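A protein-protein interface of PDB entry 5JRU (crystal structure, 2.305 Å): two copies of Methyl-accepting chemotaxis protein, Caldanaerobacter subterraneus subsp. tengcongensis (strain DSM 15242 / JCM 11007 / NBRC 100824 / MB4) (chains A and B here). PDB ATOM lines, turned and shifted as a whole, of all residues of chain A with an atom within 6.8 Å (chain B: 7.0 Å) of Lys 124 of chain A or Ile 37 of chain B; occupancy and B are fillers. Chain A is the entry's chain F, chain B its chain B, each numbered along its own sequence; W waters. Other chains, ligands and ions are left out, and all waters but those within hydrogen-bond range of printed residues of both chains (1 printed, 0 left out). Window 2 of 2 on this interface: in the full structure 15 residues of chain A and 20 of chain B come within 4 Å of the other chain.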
ATOM      1  N   PRO A 121       3.134  28.958 -21.998  1.00  0.00           N
ATOM      2  CA  PRO A 121       3.140  27.489 -22.029  1.00  0.00           C
ATOM      3  C   PRO A 121       3.770  26.909 -20.761  1.00  0.00           C
ATOM      4  O   PRO A 121       4.913  27.177 -20.515  1.00  0.00           O
ATOM      5  CB  PRO A 121       3.945  27.162 -23.296  1.00  0.00           C
ATOM      6  CG  PRO A 121       4.791  28.408 -23.588  1.00  0.00           C
ATOM      7  CD  PRO A 121       4.057  29.578 -22.982  1.00  0.00           C
ATOM      8  N   VAL A 122       2.979  26.226 -19.923  1.00  0.00           N
ATOM      9  CA  VAL A 122       3.434  25.734 -18.629  1.00  0.00           C
ATOM     10  C   VAL A 122       3.779  24.251 -18.636  1.00  0.00           C
ATOM     11  O   VAL A 122       4.369  23.753 -17.679  1.00  0.00           O
ATOM     12  CB  VAL A 122       2.381  25.979 -17.504  1.00  0.00           C
ATOM     13  CG1 VAL A 122       2.213  27.444 -17.258  1.00  0.00           C
ATOM     14  CG2 VAL A 122       1.041  25.313 -17.824  1.00  0.00           C
ATOM     15  N   ALA A 123       3.346  23.537 -19.666  1.00  0.00           N
ATOM     16  CA  ALA A 123       3.580  22.099 -19.749  1.00  0.00           C
ATOM     17  C   ALA A 123       3.626  21.699 -21.216  1.00  0.00           C
ATOM     18  O   ALA A 123       3.360  22.520 -22.087  1.00  0.00           O
ATOM     19  CB  ALA A 123       2.494  21.324 -19.004  1.00  0.00           C
ATOM     20  N   LYS A 124       4.004  20.463 -21.491  1.00  0.00           N
ATOM     21  CA  LYS A 124       4.052  20.002 -22.866  1.00  0.00           C
ATOM     22  C   LYS A 124       2.700  20.168 -23.575  1.00  0.00           C
ATOM     23  O   LYS A 124       2.661  20.480 -24.775  1.00  0.00           O
ATOM     24  CB  LYS A 124       4.565  18.555 -22.941  1.00  0.00           C
ATOM     25  CG  LYS A 124       6.022  18.472 -23.495  1.00  0.00           C
ATOM     26  CD  LYS A 124       6.747  17.109 -23.253  1.00  0.00           C
ATOM     27  CE  LYS A 124       7.892  17.303 -22.271  1.00  0.00           C
ATOM     28  NZ  LYS A 124       8.396  18.695 -22.481  1.00  0.00           N
ATOM     29  N   ASP A 125       1.598  20.039 -22.838  1.00  0.00           N
ATOM     30  CA  ASP A 125       0.276  20.138 -23.450  1.00  0.00           C
ATOM     31  C   ASP A 125      -0.681  21.148 -22.775  1.00  0.00           C
ATOM     32  O   ASP A 125      -1.891  20.959 -22.791  1.00  0.00           O
ATOM     33  CB  ASP A 125      -0.364  18.754 -23.463  1.00  0.00           C
ATOM     34  CG  ASP A 125      -0.505  18.154 -22.056  1.00  0.00           C
ATOM     35  OD1 ASP A 125      -0.259  18.878 -21.054  1.00  0.00           O
ATOM     36  OD2 ASP A 125      -0.857  16.948 -21.964  1.00  0.00           O
ATOM     37  N   ALA A 126      -0.145  22.215 -22.190  1.00  0.00           N
ATOM     38  CA  ALA A 126      -0.992  23.205 -21.541  1.00  0.00           C
ATOM     39  C   ALA A 126      -0.397  24.611 -21.451  1.00  0.00           C
ATOM     40  O   ALA A 126       0.815  24.795 -21.287  1.00  0.00           O
ATOM     41  CB  ALA A 126      -1.372  22.732 -20.118  1.00  0.00           C
ATOM     42  N   ASN A 180      -3.264  17.653 -27.859  1.00  0.00           N
ATOM     43  CA  ASN A 180      -1.947  17.455 -28.505  1.00  0.00           C
ATOM     44  C   ASN A 180      -0.900  18.405 -27.943  1.00  0.00           C
ATOM     45  O   ASN A 180      -1.244  19.445 -27.400  1.00  0.00           O
ATOM     46  CB  ASN A 180      -2.063  17.627 -30.017  1.00  0.00           C
ATOM     47  CG  ASN A 180      -3.120  16.707 -30.622  1.00  0.00           C
ATOM     48  OD1 ASN A 180      -4.292  17.076 -30.735  1.00  0.00           O
ATOM     49  ND2 ASN A 180      -2.713  15.497 -30.992  1.00  0.00           N
ATOM     50  N   PRO A 181       0.388  18.085 -28.092  1.00  0.00           N
ATOM     51  CA  PRO A 181       1.368  19.028 -27.535  1.00  0.00           C
ATOM     52  C   PRO A 181       1.340  20.458 -28.123  1.00  0.00           C
ATOM     53  O   PRO A 181       0.932  20.695 -29.275  1.00  0.00           O
ATOM     54  CB  PRO A 181       2.708  18.361 -27.859  1.00  0.00           C
ATOM     55  CG  PRO A 181       2.382  16.912 -28.006  1.00  0.00           C
ATOM     56  CD  PRO A 181       1.029  16.885 -28.645  1.00  0.00           C
ATOM     57  N   VAL A 182       1.729  21.412 -27.280  1.00  0.00           N
ATOM     58  CA  VAL A 182       1.836  22.806 -27.684  1.00  0.00           C
ATOM     59  C   VAL A 182       2.915  22.931 -28.733  1.00  0.00           C
ATOM     60  O   VAL A 182       2.708  23.536 -29.764  1.00  0.00           O
ATOM     61  CB  VAL A 182       2.174  23.740 -26.503  1.00  0.00           C
ATOM     62  CG1 VAL A 182       2.348  25.189 -27.006  1.00  0.00           C
ATOM     63  CG2 VAL A 182       1.099  23.644 -25.397  1.00  0.00           C
ATOM     64  N   PHE A 183       4.085  22.372 -28.446  1.00  0.00           N
ATOM     65  CA  PHE A 183       5.173  22.366 -29.415  1.00  0.00           C
ATOM     66  C   PHE A 183       5.552  20.961 -29.787  1.00  0.00           C
ATOM     67  O   PHE A 183       6.631  20.495 -29.468  1.00  0.00           O
ATOM     68  CB  PHE A 183       6.376  23.106 -28.856  1.00  0.00           C
ATOM     69  CG  PHE A 183       6.065  24.495 -28.443  1.00  0.00           C
ATOM     70  CD1 PHE A 183       5.785  25.458 -29.393  1.00  0.00           C
ATOM     71  CD2 PHE A 183       5.952  24.821 -27.111  1.00  0.00           C
ATOM     72  CE1 PHE A 183       5.486  26.738 -29.024  1.00  0.00           C
ATOM     73  CE2 PHE A 183       5.631  26.089 -26.730  1.00  0.00           C
ATOM     74  CZ  PHE A 183       5.397  27.058 -27.691  1.00  0.00           C
ATOM     75  N   GLU A 184       4.689  20.305 -30.533  1.00  0.00           N
ATOM     76  CA  GLU A 184       4.943  18.925 -30.868  1.00  0.00           C
ATOM     77  C   GLU A 184       6.092  18.778 -31.856  1.00  0.00           C
ATOM     78  O   GLU A 184       6.184  19.510 -32.839  1.00  0.00           O
ATOM     79  CB  GLU A 184       3.671  18.301 -31.453  1.00  0.00           C
ATOM     80  CG  GLU A 184       3.813  16.845 -31.782  1.00  0.00           C
ATOM     81  CD  GLU A 184       2.498  16.221 -32.193  1.00  0.00           C
ATOM     82  OE1 GLU A 184       1.586  16.961 -32.639  1.00  0.00           O
ATOM     83  OE2 GLU A 184       2.381  14.983 -32.064  1.00  0.00           O
ATOM     84  N   LYS B   2      15.905  27.963 -24.013  1.00  0.00           N
ATOM     85  CA  LYS B   2      14.611  27.519 -23.522  1.00  0.00           C
ATOM     86  C   LYS B   2      14.357  26.028 -23.842  1.00  0.00           C
ATOM     87  O   LYS B   2      14.747  25.502 -24.897  1.00  0.00           O
ATOM     88  CB  LYS B   2      13.540  28.437 -24.133  1.00  0.00           C
ATOM     89  CG  LYS B   2      13.581  29.885 -23.553  1.00  0.00           C
ATOM     90  CD  LYS B   2      13.076  29.741 -22.103  1.00  0.00           C
ATOM     91  CE  LYS B   2      13.438  30.844 -21.156  1.00  0.00           C
ATOM     92  NZ  LYS B   2      13.089  30.344 -19.809  1.00  0.00           N
ATOM     93  N   GLY B   3      13.706  25.339 -22.918  1.00  0.00           N
ATOM     94  CA  GLY B   3      13.411  23.946 -23.126  1.00  0.00           C
ATOM     95  C   GLY B   3      12.638  23.634 -24.394  1.00  0.00           C
ATOM     96  O   GLY B   3      12.803  22.564 -24.966  1.00  0.00           O
ATOM     97  N   THR B   4      11.795  24.561 -24.831  1.00  0.00           N
ATOM     98  CA  THR B   4      11.002  24.365 -26.037  1.00  0.00           C
ATOM     99  C   THR B   4      11.853  23.886 -27.199  1.00  0.00           C
ATOM    100  O   THR B   4      11.613  22.819 -27.765  1.00  0.00           O
ATOM    101  CB  THR B   4      10.342  25.677 -26.525  1.00  0.00           C
ATOM    102  OG1 THR B   4       9.417  26.186 -25.554  1.00  0.00           O
ATOM    103  CG2 THR B   4       9.638  25.446 -27.841  1.00  0.00           C
ATOM    104  N   VAL B   6      15.090  23.151 -27.074  1.00  0.00           N
ATOM    105  CA  VAL B   6      16.046  22.079 -26.697  1.00  0.00           C
ATOM    106  C   VAL B   6      15.401  20.708 -26.792  1.00  0.00           C
ATOM    107  O   VAL B   6      16.057  19.753 -27.224  1.00  0.00           O
ATOM    108  CB  VAL B   6      16.659  22.269 -25.299  1.00  0.00           C
ATOM    109  CG1 VAL B   6      17.556  21.053 -24.912  1.00  0.00           C
ATOM    110  CG2 VAL B   6      17.489  23.528 -25.286  1.00  0.00           C
ATOM    111  N   GLY B   7      14.132  20.613 -26.373  1.00  0.00           N
ATOM    112  CA  GLY B   7      13.376  19.371 -26.469  1.00  0.00           C
ATOM    113  C   GLY B   7      13.278  18.922 -27.911  1.00  0.00           C
ATOM    114  O   GLY B   7      13.552  17.775 -28.266  1.00  0.00           O
ATOM    115  N   THR B   8      12.990  19.874 -28.778  1.00  0.00           N
ATOM    116  CA  THR B   8      12.991  19.608 -30.207  1.00  0.00           C
ATOM    117  C   THR B   8      14.372  19.129 -30.739  1.00  0.00           C
ATOM    118  O   THR B   8      14.438  18.178 -31.512  1.00  0.00           O
ATOM    119  CB  THR B   8      12.547  20.866 -30.934  1.00  0.00           C
ATOM    120  OG1 THR B   8      11.192  21.127 -30.560  1.00  0.00           O
ATOM    121  CG2 THR B   8      12.669  20.717 -32.448  1.00  0.00           C
ATOM    122  N   ILE B  10      16.770  17.513 -29.168  1.00  0.00           N
ATOM    123  CA  ILE B  10      16.971  16.146 -28.698  1.00  0.00           C
ATOM    124  C   ILE B  10      16.201  15.190 -29.605  1.00  0.00           C
ATOM    125  O   ILE B  10      16.774  14.232 -30.114  1.00  0.00           O
ATOM    126  CB  ILE B  10      16.488  15.909 -27.234  1.00  0.00           C
ATOM    127  CG1 ILE B  10      17.030  16.935 -26.218  1.00  0.00           C
ATOM    128  CG2 ILE B  10      16.780  14.496 -26.828  1.00  0.00           C
ATOM    129  CD1 ILE B  10      18.480  17.236 -26.312  1.00  0.00           C
ATOM    130  N   LYS B  11      14.932  15.494 -29.876  1.00  0.00           N
ATOM    131  CA  LYS B  11      14.150  14.571 -30.676  1.00  0.00           C
ATOM    132  C   LYS B  11      14.666  14.510 -32.070  1.00  0.00           C
ATOM    133  O   LYS B  11      14.688  13.421 -32.635  1.00  0.00           O
ATOM    134  CB  LYS B  11      12.644  14.895 -30.662  1.00  0.00           C
ATOM    135  CG  LYS B  11      11.984  14.612 -29.300  1.00  0.00           C
ATOM    136  CD  LYS B  11      11.277  15.825 -28.723  1.00  0.00           C
ATOM    137  CE  LYS B  11      10.341  15.480 -27.562  1.00  0.00           C
ATOM    138  NZ  LYS B  11       9.706  16.746 -27.070  1.00  0.00           N
ATOM    139  N   LEU B  26      23.285  12.214 -23.604  1.00  0.00           N
ATOM    140  CA  LEU B  26      22.649  12.848 -22.471  1.00  0.00           C
ATOM    141  C   LEU B  26      23.314  12.397 -21.167  1.00  0.00           C
ATOM    142  O   LEU B  26      23.617  13.214 -20.324  1.00  0.00           O
ATOM    143  CB  LEU B  26      21.141  12.579 -22.436  1.00  0.00           C
ATOM    144  CG  LEU B  26      20.220  13.709 -22.963  1.00  0.00           C
ATOM    145  CD1 LEU B  26      20.528  14.099 -24.378  1.00  0.00           C
ATOM    146  CD2 LEU B  26      18.758  13.379 -22.797  1.00  0.00           C
ATOM    147  N   TRP B  31      22.627  14.088 -17.443  1.00  0.00           N
ATOM    148  CA  TRP B  31      21.188  14.164 -17.525  1.00  0.00           C
ATOM    149  C   TRP B  31      20.636  12.755 -17.584  1.00  0.00           C
ATOM    150  O   TRP B  31      21.294  11.856 -18.137  1.00  0.00           O
ATOM    151  CB  TRP B  31      20.724  14.893 -18.771  1.00  0.00           C
ATOM    152  CG  TRP B  31      21.103  16.276 -18.948  1.00  0.00           C
ATOM    153  CD1 TRP B  31      21.978  17.017 -18.217  1.00  0.00           C
ATOM    154  CD2 TRP B  31      20.577  17.135 -19.947  1.00  0.00           C
ATOM    155  NE1 TRP B  31      22.036  18.294 -18.719  1.00  0.00           N
ATOM    156  CE2 TRP B  31      21.186  18.388 -19.785  1.00  0.00           C
ATOM    157  CE3 TRP B  31      19.641  16.960 -20.976  1.00  0.00           C
ATOM    158  CZ2 TRP B  31      20.898  19.463 -20.616  1.00  0.00           C
ATOM    159  CZ3 TRP B  31      19.354  18.023 -21.799  1.00  0.00           C
ATOM    160  CH2 TRP B  31      19.988  19.257 -21.624  1.00  0.00           C
ATOM    161  N   ASP B  34      16.370  10.265 -20.554  1.00  0.00           N
ATOM    162  CA  ASP B  34      14.983  10.570 -20.866  1.00  0.00           C
ATOM    163  C   ASP B  34      14.501  11.849 -20.179  1.00  0.00           C
ATOM    164  O   ASP B  34      13.314  11.948 -19.829  1.00  0.00           O
ATOM    165  CB  ASP B  34      14.093   9.401 -20.462  1.00  0.00           C
ATOM    166  CG  ASP B  34      14.264   9.016 -18.982  1.00  0.00           C
ATOM    167  OD1 ASP B  34      15.202   9.547 -18.327  1.00  0.00           O
ATOM    168  OD2 ASP B  34      13.457   8.178 -18.481  1.00  0.00           O
ATOM    169  N   ARG B  35      15.409  12.801 -19.942  1.00  0.00           N
ATOM    170  CA  ARG B  35      15.014  14.027 -19.237  1.00  0.00           C
ATOM    171  C   ARG B  35      13.737  14.665 -19.794  1.00  0.00           C
ATOM    172  O   ARG B  35      13.597  14.827 -20.991  1.00  0.00           O
ATOM    173  CB  ARG B  35      16.148  15.056 -19.246  1.00  0.00           C
ATOM    174  CG  ARG B  35      15.771  16.350 -18.504  1.00  0.00           C
ATOM    175  CD  ARG B  35      16.938  17.321 -18.458  1.00  0.00           C
ATOM    176  NE  ARG B  35      16.635  18.576 -17.762  1.00  0.00           N
ATOM    177  CZ  ARG B  35      17.561  19.445 -17.369  1.00  0.00           C
ATOM    178  NH1 ARG B  35      18.838  19.184 -17.602  1.00  0.00           N
ATOM    179  NH2 ARG B  35      17.226  20.574 -16.772  1.00  0.00           N
ATOM    180  N   VAL B  36      12.795  14.968 -18.901  1.00  0.00           N
ATOM    181  CA  VAL B  36      11.548  15.625 -19.254  1.00  0.00           C
ATOM    182  C   VAL B  36      11.869  17.131 -19.212  1.00  0.00           C
ATOM    183  O   VAL B  36      12.355  17.639 -18.198  1.00  0.00           O
ATOM    184  CB  VAL B  36      10.425  15.217 -18.250  1.00  0.00           C
ATOM    185  CG1 VAL B  36       9.090  15.927 -18.519  1.00  0.00           C
ATOM    186  CG2 VAL B  36      10.231  13.684 -18.264  1.00  0.00           C
ATOM    187  N   ILE B  37      11.654  17.838 -20.321  1.00  0.00           N
ATOM    188  CA  ILE B  37      11.988  19.259 -20.400  1.00  0.00           C
ATOM    189  C   ILE B  37      10.747  20.117 -20.647  1.00  0.00           C
ATOM    190  O   ILE B  37      10.060  19.887 -21.619  1.00  0.00           O
ATOM    191  CB  ILE B  37      12.995  19.518 -21.524  1.00  0.00           C
ATOM    192  CG1 ILE B  37      14.241  18.641 -21.373  1.00  0.00           C
ATOM    193  CG2 ILE B  37      13.352  20.953 -21.527  1.00  0.00           C
ATOM    194  CD1 ILE B  37      15.175  18.679 -22.589  1.00  0.00           C
ATOM    195  N   THR B  38      10.448  21.095 -19.808  1.00  0.00           N
ATOM    196  CA  THR B  38       9.208  21.864 -20.028  1.00  0.00           C
ATOM    197  C   THR B  38       9.483  23.011 -20.996  1.00  0.00           C
ATOM    198  O   THR B  38      10.651  23.336 -21.252  1.00  0.00           O
ATOM    199  CB  THR B  38       8.576  22.401 -18.718  1.00  0.00           C
ATOM    200  OG1 THR B  38       9.385  23.433 -18.141  1.00  0.00           O
ATOM    201  CG2 THR B  38       8.395  21.273 -17.733  1.00  0.00           C
ATOM    202  N   PRO B  39       8.429  23.575 -21.589  1.00  0.00           N
ATOM    203  CA  PRO B  39       8.715  24.593 -22.616  1.00  0.00           C
ATOM    204  C   PRO B  39       9.503  25.788 -22.094  1.00  0.00           C
ATOM    205  O   PRO B  39      10.311  26.354 -22.846  1.00  0.00           O
ATOM    206  CB  PRO B  39       7.316  25.035 -23.075  1.00  0.00           C
ATOM    207  CG  PRO B  39       6.429  23.846 -22.783  1.00  0.00           C
ATOM    208  CD  PRO B  39       7.008  23.165 -21.575  1.00  0.00           C
ATOM    209  N   LEU B  40       9.312  26.169 -20.836  1.00  0.00           N
ATOM    210  CA  LEU B  40       9.920  27.407 -20.378  1.00  0.00           C
ATOM    211  C   LEU B  40      11.132  27.240 -19.459  1.00  0.00           C
ATOM    212  O   LEU B  40      11.712  28.238 -19.034  1.00  0.00           O
ATOM    213  CB  LEU B  40       8.880  28.269 -19.671  1.00  0.00           C
ATOM    214  CG  LEU B  40       7.814  28.857 -20.597  1.00  0.00           C
ATOM    215  CD1 LEU B  40       6.850  29.766 -19.852  1.00  0.00           C
ATOM    216  CD2 LEU B  40       8.442  29.621 -21.728  1.00  0.00           C
ATOM    217  N   GLU B  41      11.550  26.021 -19.142  1.00  0.00           N
ATOM    218  CA  GLU B  41      12.751  25.928 -18.296  1.00  0.00           C
ATOM    219  C   GLU B  41      14.041  26.313 -19.003  1.00  0.00           C
ATOM    220  O   GLU B  41      14.187  26.167 -20.223  1.00  0.00           O
ATOM    221  CB  GLU B  41      12.882  24.548 -17.683  1.00  0.00           C
ATOM    222  CG  GLU B  41      13.226  23.500 -18.615  1.00  0.00           C
ATOM    223  CD  GLU B  41      13.666  22.263 -17.892  1.00  0.00           C
ATOM    224  OE1 GLU B  41      14.633  22.347 -17.096  1.00  0.00           O
ATOM    225  OE2 GLU B  41      13.044  21.213 -18.133  1.00  0.00           O
ATOM    226  N   ASP B  42      14.996  26.779 -18.218  1.00  0.00           N
ATOM    227  CA  ASP B  42      16.267  27.246 -18.763  1.00  0.00           C
ATOM    228  C   ASP B  42      17.337  26.172 -18.800  1.00  0.00           C
ATOM    229  O   ASP B  42      17.766  25.660 -17.772  1.00  0.00           O
ATOM    230  CB  ASP B  42      16.765  28.424 -17.949  1.00  0.00           C
ATOM    231  CG  ASP B  42      15.916  29.649 -18.149  1.00  0.00           C
ATOM    232  OD1 ASP B  42      15.517  29.894 -19.310  1.00  0.00           O
ATOM    233  OD2 ASP B  42      15.655  30.360 -17.149  1.00  0.00           O
ATOM    234  N   ILE B  43      17.778  25.834 -20.001  1.00  0.00           N
ATOM    235  CA  ILE B  43      18.730  24.752 -20.160  1.00  0.00           C
ATOM    236  C   ILE B  43      20.087  25.376 -20.400  1.00  0.00           C
ATOM    237  O   ILE B  43      20.204  26.275 -21.227  1.00  0.00           O
ATOM    238  CB  ILE B  43      18.316  23.833 -21.327  1.00  0.00           C
ATOM    239  CG1 ILE B  43      16.816  23.457 -21.258  1.00  0.00           C
ATOM    240  CG2 ILE B  43      19.260  22.650 -21.459  1.00  0.00           C
ATOM    241  CD1 ILE B  43      16.336  22.653 -20.042  1.00  0.00           C
HETATM  242  O   HOH W   1       7.039  25.191 -19.267  1.00  0.00           O
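The side-chain amino group of Lys 124 of chain A sits close to the backbone carbonyl oxygen of Ile 37 of chain B (2.2 Å).
O of Leu 40 of chain B lies within hydrogen-bond range of NZ of Lys 2 of chain B, at 2.6 Å. OG1 of Thr 8 of chain B lies within hydrogen-bond range of O of Thr 4 of chain B. O of Pro 39 of chain B sits at hydrogen-bond distance from OG1 of Thr 4 of chain B (2.9 Å). N of Val 182 of chain A is in hydrogen-bond range of O of Lys 124 of chain A (2.8 Å).
Among the printed residues, merely in contact across the chains: Pro 121 of chain A with Leu 40 of chain B, Ala 123 of chain A with Pro 39 of chain B, Phe 183 of chain A with Thr 4 of chain B and Pro 121 of chain A with Pro 39 of chain B.
Of chain B, only Ile 37 comes within 4 Å of Lys 124 of chain A. Of the printed residues of chain B, Phe 183 of chain A touches Thr 4 (3.7 Å). Printed residues of chain A within 4 Å of Thr 4 of chain B: Phe 183 (3.7 Å). Of the printed residues of chain A, Leu 40 of chain B touches Pro 121. Ile 43 of chain B touches none of the printed residues of chain A.
Of the 11 printed residues of chain A, 4 touch a printed residue of chain B. Along chain A the printed residues that touch a printed residue of chain B span positions 121 to 183. Among the printed residues, 5 pairs touch across the chains. Among the printed residues, no Asp or Glu carboxylate lies within 4 Å of a Lys or Arg side-chain nitrogen of the other chain.
No position is printed for both chains.
Water W1 lies within hydrogen-bond range of N of Leu 40 of chain B, OG1 of Thr 38 of chain B, O of Pro 121 of chain A and O of Val 122 of chain A.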
